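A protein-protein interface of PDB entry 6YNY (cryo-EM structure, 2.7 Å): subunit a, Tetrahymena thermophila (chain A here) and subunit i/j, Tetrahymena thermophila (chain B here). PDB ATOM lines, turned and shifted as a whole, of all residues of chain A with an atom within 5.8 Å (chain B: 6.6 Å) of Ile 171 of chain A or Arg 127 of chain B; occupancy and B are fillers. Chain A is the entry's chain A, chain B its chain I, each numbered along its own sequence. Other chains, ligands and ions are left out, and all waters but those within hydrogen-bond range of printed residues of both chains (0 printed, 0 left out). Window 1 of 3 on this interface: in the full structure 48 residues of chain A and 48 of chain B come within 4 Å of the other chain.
Among the printed residues, pairs that only touch across the chains: Pro 167 of chain A with Arg 127 of chain B, Asp 168 of chain A with Lys 126 of chain B, Met 169 of chain A with Asp 130 of chain B, Ile 171 of chain A with Arg 127 of chain B and Pro 167 of chain A with Gly 129 of chain B.
Of the printed residues of chain B, Pro 167 of chain A touches Arg 127 and Gly 129.
Of the printed residues of chain B, Asp 168 of chain A touches Lys 126 (3.6 Å) and Arg 127 (2.8 Å).
Printed residues of chain B within 4 Å of Met 169 of chain A: Lys 126 (2.9 Å) and Asp 130 (3.6 Å).
Cys 170 of chain A touches none of the printed residues of chain B.
Of chain B, only Arg 127 comes within 4 Å of Ile 171 of chain A.
Asp 112 of chain B touches none of the printed residues of chain A.
Of chain A, only Pro 167, Asp 168 and Ile 171 come within 4 Å of Arg 127 of chain B.
Printed residues of chain A within 4 Å of Asp 130 of chain B: Met 169 (3.6 Å).
The nearest printed residue of chain B that does not touch Asp 168 of chain A is Gly 129 of chain B (4.3 Å).
The side-chain carboxylate (OD1) of Asp 168 of chain A is in salt-bridge range of the guanidinium group (NE) of Arg 127 of chain B, at 2.8 Å.
The backbone carbonyl oxygen (O) of Lys 126 of chain B is in hydrogen-bond range of the backbone NH (N) of Met 169 of chain A, at 2.9 Å.
Of the 9 printed residues of chain A, 4 touch a printed residue of chain B.
Printed residues of chain A that touch a printed residue of chain B: Pro 167, Asp 168, Met 169 and Ile 171.
Hydrophobic or aromatic side chains of chain A within 4 Å of the printed part of chain B: Pro 167, Met 169 and Ile 171.
Of the 11 printed residues of chain B, 4 touch a printed residue of chain A.
Among the printed residues, 7 pairs touch across the chains.
Among the printed residues, Asp or Glu carboxylates within 4 Å of a Lys or Arg side-chain nitrogen of the other chain: Asp 168 of chain A with Arg 127 of chain B.
The side-chain carboxylate of Asp 168 of chain A is in hydrogen-bond range of the side-chain hydroxyl of Tyr 64 of chain A.
NH1 of Arg 127 of chain B is in hydrogen-bond range of OH of Tyr 123 of chain B.
O of Lys 125 of chain B sits at hydrogen-bond distance from N of Asp 130 of chain B (2.7 Å).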
ATOM      1  N   TYR A  64     -10.156   3.029  16.597  1.00  0.00           N
ATOM      2  CA  TYR A  64      -9.198   4.126  16.498  1.00  0.00           C
ATOM      3  C   TYR A  64      -8.591   4.357  17.877  1.00  0.00           C
ATOM      4  O   TYR A  64      -8.967   5.262  18.624  1.00  0.00           O
ATOM      5  CB  TYR A  64      -9.860   5.386  15.959  1.00  0.00           C
ATOM      6  CG  TYR A  64     -10.623   5.192  14.677  1.00  0.00           C
ATOM      7  CD1 TYR A  64     -11.960   5.533  14.587  1.00  0.00           C
ATOM      8  CD2 TYR A  64     -10.008   4.668  13.558  1.00  0.00           C
ATOM      9  CE1 TYR A  64     -12.660   5.360  13.418  1.00  0.00           C
ATOM     10  CE2 TYR A  64     -10.700   4.489  12.384  1.00  0.00           C
ATOM     11  CZ  TYR A  64     -12.026   4.836  12.320  1.00  0.00           C
ATOM     12  OH  TYR A  64     -12.724   4.661  11.152  1.00  0.00           O
ATOM     13  N   PRO A 167     -14.471   2.929  18.895  1.00  0.00           N
ATOM     14  CA  PRO A 167     -15.017   1.952  17.955  1.00  0.00           C
ATOM     15  C   PRO A 167     -15.781   2.606  16.817  1.00  0.00           C
ATOM     16  O   PRO A 167     -16.346   3.693  16.951  1.00  0.00           O
ATOM     17  CB  PRO A 167     -15.939   1.103  18.832  1.00  0.00           C
ATOM     18  CG  PRO A 167     -16.318   1.984  19.931  1.00  0.00           C
ATOM     19  CD  PRO A 167     -15.157   2.877  20.194  1.00  0.00           C
ATOM     20  N   ASP A 168     -15.787   1.918  15.680  1.00  0.00           N
ATOM     21  CA  ASP A 168     -16.494   2.390  14.493  1.00  0.00           C
ATOM     22  C   ASP A 168     -16.684   1.210  13.558  1.00  0.00           C
ATOM     23  O   ASP A 168     -15.704   0.579  13.156  1.00  0.00           O
ATOM     24  CB  ASP A 168     -15.721   3.508  13.801  1.00  0.00           C
ATOM     25  CG  ASP A 168     -16.454   4.074  12.605  1.00  0.00           C
ATOM     26  OD1 ASP A 168     -17.627   3.710  12.395  1.00  0.00           O
ATOM     27  OD2 ASP A 168     -15.852   4.882  11.869  1.00  0.00           O
ATOM     28  N   MET A 169     -17.931   0.913  13.217  1.00  0.00           N
ATOM     29  CA  MET A 169     -18.210  -0.177  12.297  1.00  0.00           C
ATOM     30  C   MET A 169     -17.768   0.203  10.895  1.00  0.00           C
ATOM     31  O   MET A 169     -18.175   1.239  10.363  1.00  0.00           O
ATOM     32  CB  MET A 169     -19.695  -0.519  12.311  1.00  0.00           C
ATOM     33  CG  MET A 169     -20.211  -0.966  13.660  1.00  0.00           C
ATOM     34  SD  MET A 169     -19.356  -2.401  14.329  1.00  0.00           S
ATOM     35  CE  MET A 169     -19.837  -3.650  13.149  1.00  0.00           C
ATOM     36  N   CYS A 170     -16.927  -0.633  10.298  1.00  0.00           N
ATOM     37  CA  CYS A 170     -16.442  -0.367   8.954  1.00  0.00           C
ATOM     38  C   CYS A 170     -17.556  -0.614   7.948  1.00  0.00           C
ATOM     39  O   CYS A 170     -18.163  -1.687   7.927  1.00  0.00           O
ATOM     40  CB  CYS A 170     -15.235  -1.247   8.639  1.00  0.00           C
ATOM     41  SG  CYS A 170     -14.382  -0.797   7.125  1.00  0.00           S
ATOM     42  N   ILE A 171     -17.828   0.391   7.123  1.00  0.00           N
ATOM     43  CA  ILE A 171     -18.866   0.306   6.105  1.00  0.00           C
ATOM     44  C   ILE A 171     -18.191  -0.215   4.842  1.00  0.00           C
ATOM     45  O   ILE A 171     -17.471   0.510   4.158  1.00  0.00           O
ATOM     46  CB  ILE A 171     -19.554   1.653   5.885  1.00  0.00           C
ATOM     47  CG1 ILE A 171     -20.086   2.200   7.212  1.00  0.00           C
ATOM     48  CG2 ILE A 171     -20.697   1.506   4.919  1.00  0.00           C
ATOM     49  CD1 ILE A 171     -19.101   3.058   7.969  1.00  0.00           C
ATOM     50  N   LEU A 172     -18.424  -1.487   4.542  1.00  0.00           N
ATOM     51  CA  LEU A 172     -17.738  -2.200   3.479  1.00  0.00           C
ATOM     52  C   LEU A 172     -18.721  -2.611   2.392  1.00  0.00           C
ATOM     53  O   LEU A 172     -19.940  -2.526   2.551  1.00  0.00           O
ATOM     54  CB  LEU A 172     -17.024  -3.437   4.031  1.00  0.00           C
ATOM     55  CG  LEU A 172     -15.911  -3.172   5.039  1.00  0.00           C
ATOM     56  CD1 LEU A 172     -15.563  -4.433   5.798  1.00  0.00           C
ATOM     57  CD2 LEU A 172     -14.694  -2.635   4.337  1.00  0.00           C
ATOM     58  N   VAL A 173     -18.161  -3.068   1.279  1.00  0.00           N
ATOM     59  CA  VAL A 173     -18.933  -3.556   0.145  1.00  0.00           C
ATOM     60  C   VAL A 173     -19.027  -5.072   0.147  1.00  0.00           C
ATOM     61  O   VAL A 173     -20.098  -5.637  -0.066  1.00  0.00           O
ATOM     62  CB  VAL A 173     -18.313  -3.048  -1.175  1.00  0.00           C
ATOM     63  CG1 VAL A 173     -19.083  -3.584  -2.360  1.00  0.00           C
ATOM     64  CG2 VAL A 173     -18.264  -1.545  -1.199  1.00  0.00           C
ATOM     65  N   THR A 175     -18.932  -7.185   2.488  1.00  0.00           N
ATOM     66  CA  THR A 175     -19.658  -7.812   3.583  1.00  0.00           C
ATOM     67  C   THR A 175     -21.086  -8.154   3.189  1.00  0.00           C
ATOM     68  O   THR A 175     -21.637  -9.151   3.667  1.00  0.00           O
ATOM     69  CB  THR A 175     -19.653  -6.903   4.807  1.00  0.00           C
ATOM     70  OG1 THR A 175     -20.071  -5.586   4.433  1.00  0.00           O
ATOM     71  CG2 THR A 175     -18.273  -6.847   5.410  1.00  0.00           C
ATOM     72  N   ASP B 112     -29.940   0.539   3.450  1.00  0.00           N
ATOM     73  CA  ASP B 112     -28.901   1.477   3.039  1.00  0.00           C
ATOM     74  C   ASP B 112     -28.895   1.712   1.535  1.00  0.00           C
ATOM     75  O   ASP B 112     -28.487   2.786   1.081  1.00  0.00           O
ATOM     76  CB  ASP B 112     -27.536   0.967   3.490  1.00  0.00           C
ATOM     77  CG  ASP B 112     -27.470   0.717   4.980  1.00  0.00           C
ATOM     78  OD1 ASP B 112     -28.470   0.989   5.675  1.00  0.00           O
ATOM     79  OD2 ASP B 112     -26.417   0.243   5.456  1.00  0.00           O
ATOM     80  N   SER B 117     -28.283   6.740   3.608  1.00  0.00           N
ATOM     81  CA  SER B 117     -28.249   6.197   4.958  1.00  0.00           C
ATOM     82  C   SER B 117     -27.780   7.190   6.018  1.00  0.00           C
ATOM     83  O   SER B 117     -28.289   7.111   7.149  1.00  0.00           O
ATOM     84  CB  SER B 117     -27.371   4.938   4.967  1.00  0.00           C
ATOM     85  OG  SER B 117     -26.048   5.221   4.556  1.00  0.00           O
ATOM     86  N   PRO B 122     -30.120   4.187  11.858  1.00  0.00           N
ATOM     87  CA  PRO B 122     -29.183   3.058  11.965  1.00  0.00           C
ATOM     88  C   PRO B 122     -27.751   3.406  11.620  1.00  0.00           C
ATOM     89  O   PRO B 122     -26.838   2.703  12.069  1.00  0.00           O
ATOM     90  CB  PRO B 122     -29.759   2.035  10.980  1.00  0.00           C
ATOM     91  CG  PRO B 122     -31.169   2.400  10.839  1.00  0.00           C
ATOM     92  CD  PRO B 122     -31.227   3.877  10.945  1.00  0.00           C
ATOM     93  N   TYR B 123     -27.516   4.456  10.837  1.00  0.00           N
ATOM     94  CA  TYR B 123     -26.147   4.838  10.515  1.00  0.00           C
ATOM     95  C   TYR B 123     -25.417   5.347  11.750  1.00  0.00           C
ATOM     96  O   TYR B 123     -24.230   5.063  11.938  1.00  0.00           O
ATOM     97  CB  TYR B 123     -26.155   5.898   9.415  1.00  0.00           C
ATOM     98  CG  TYR B 123     -24.795   6.324   8.931  1.00  0.00           C
ATOM     99  CD1 TYR B 123     -24.071   5.534   8.056  1.00  0.00           C
ATOM    100  CD2 TYR B 123     -24.241   7.526   9.332  1.00  0.00           C
ATOM    101  CE1 TYR B 123     -22.837   5.920   7.607  1.00  0.00           C
ATOM    102  CE2 TYR B 123     -23.005   7.921   8.886  1.00  0.00           C
ATOM    103  CZ  TYR B 123     -22.307   7.116   8.023  1.00  0.00           C
ATOM    104  OH  TYR B 123     -21.071   7.507   7.576  1.00  0.00           O
ATOM    105  N   LEU B 124     -26.113   6.092  12.606  1.00  0.00           N
ATOM    106  CA  LEU B 124     -25.494   6.603  13.822  1.00  0.00           C
ATOM    107  C   LEU B 124     -25.015   5.469  14.716  1.00  0.00           C
ATOM    108  O   LEU B 124     -23.955   5.568  15.345  1.00  0.00           O
ATOM    109  CB  LEU B 124     -26.483   7.488  14.571  1.00  0.00           C
ATOM    110  CG  LEU B 124     -26.235   8.988  14.581  1.00  0.00           C
ATOM    111  CD1 LEU B 124     -25.961   9.506  13.202  1.00  0.00           C
ATOM    112  CD2 LEU B 124     -27.442   9.661  15.165  1.00  0.00           C
ATOM    113  N   LYS B 125     -25.783   4.385  14.789  1.00  0.00           N
ATOM    114  CA  LYS B 125     -25.390   3.262  15.629  1.00  0.00           C
ATOM    115  C   LYS B 125     -24.149   2.569  15.087  1.00  0.00           C
ATOM    116  O   LYS B 125     -23.289   2.130  15.860  1.00  0.00           O
ATOM    117  CB  LYS B 125     -26.544   2.272  15.750  1.00  0.00           C
ATOM    118  CG  LYS B 125     -27.758   2.829  16.449  1.00  0.00           C
ATOM    119  CD  LYS B 125     -28.724   1.739  16.851  1.00  0.00           C
ATOM    120  CE  LYS B 125     -29.263   0.995  15.656  1.00  0.00           C
ATOM    121  NZ  LYS B 125     -30.235  -0.031  16.063  1.00  0.00           N
ATOM    122  N   LYS B 126     -24.035   2.457  13.765  1.00  0.00           N
ATOM    123  CA  LYS B 126     -22.858   1.824  13.186  1.00  0.00           C
ATOM    124  C   LYS B 126     -21.603   2.643  13.451  1.00  0.00           C
ATOM    125  O   LYS B 126     -20.535   2.083  13.716  1.00  0.00           O
ATOM    126  CB  LYS B 126     -23.063   1.612  11.690  1.00  0.00           C
ATOM    127  CG  LYS B 126     -23.922   0.410  11.362  1.00  0.00           C
ATOM    128  CD  LYS B 126     -23.955   0.128   9.877  1.00  0.00           C
ATOM    129  CE  LYS B 126     -25.242   0.586   9.245  1.00  0.00           C
ATOM    130  NZ  LYS B 126     -26.396  -0.225   9.709  1.00  0.00           N
ATOM    131  N   ARG B 127     -21.710   3.968  13.386  1.00  0.00           N
ATOM    132  CA  ARG B 127     -20.560   4.816  13.652  1.00  0.00           C
ATOM    133  C   ARG B 127     -20.264   4.937  15.139  1.00  0.00           C
ATOM    134  O   ARG B 127     -19.150   5.322  15.507  1.00  0.00           O
ATOM    135  CB  ARG B 127     -20.782   6.202  13.054  1.00  0.00           C
ATOM    136  CG  ARG B 127     -21.192   6.191  11.597  1.00  0.00           C
ATOM    137  CD  ARG B 127     -20.239   5.404  10.726  1.00  0.00           C
ATOM    138  NE  ARG B 127     -18.851   5.803  10.922  1.00  0.00           N
ATOM    139  CZ  ARG B 127     -18.305   6.882  10.379  1.00  0.00           C
ATOM    140  NH1 ARG B 127     -19.024   7.677   9.608  1.00  0.00           N
ATOM    141  NH2 ARG B 127     -17.037   7.169  10.612  1.00  0.00           N
ATOM    142  N   ALA B 128     -21.231   4.628  15.995  1.00  0.00           N
ATOM    143  CA  ALA B 128     -21.021   4.595  17.433  1.00  0.00           C
ATOM    144  C   ALA B 128     -20.566   3.227  17.925  1.00  0.00           C
ATOM    145  O   ALA B 128     -20.619   2.966  19.129  1.00  0.00           O
ATOM    146  CB  ALA B 128     -22.298   5.008  18.160  1.00  0.00           C
ATOM    147  N   GLY B 129     -20.128   2.355  17.024  1.00  0.00           N
ATOM    148  CA  GLY B 129     -19.675   1.033  17.409  1.00  0.00           C
ATOM    149  C   GLY B 129     -20.779   0.015  17.561  1.00  0.00           C
ATOM    150  O   GLY B 129     -20.709  -0.838  18.453  1.00  0.00           O
ATOM    151  N   ASP B 130     -21.797   0.078  16.711  1.00  0.00           N
ATOM    152  CA  ASP B 130     -22.960  -0.799  16.804  1.00  0.00           C
ATOM    153  C   ASP B 130     -23.520  -0.780  18.224  1.00  0.00           C
ATOM    154  O   ASP B 130     -23.631  -1.802  18.902  1.00  0.00           O
ATOM    155  CB  ASP B 130     -22.616  -2.219  16.365  1.00  0.00           C
ATOM    156  CG  ASP B 130     -23.832  -3.120  16.321  1.00  0.00           C
ATOM    157  OD1 ASP B 130     -24.754  -2.831  15.533  1.00  0.00           O
ATOM    158  OD2 ASP B 130     -23.867  -4.117  17.071  1.00  0.00           O
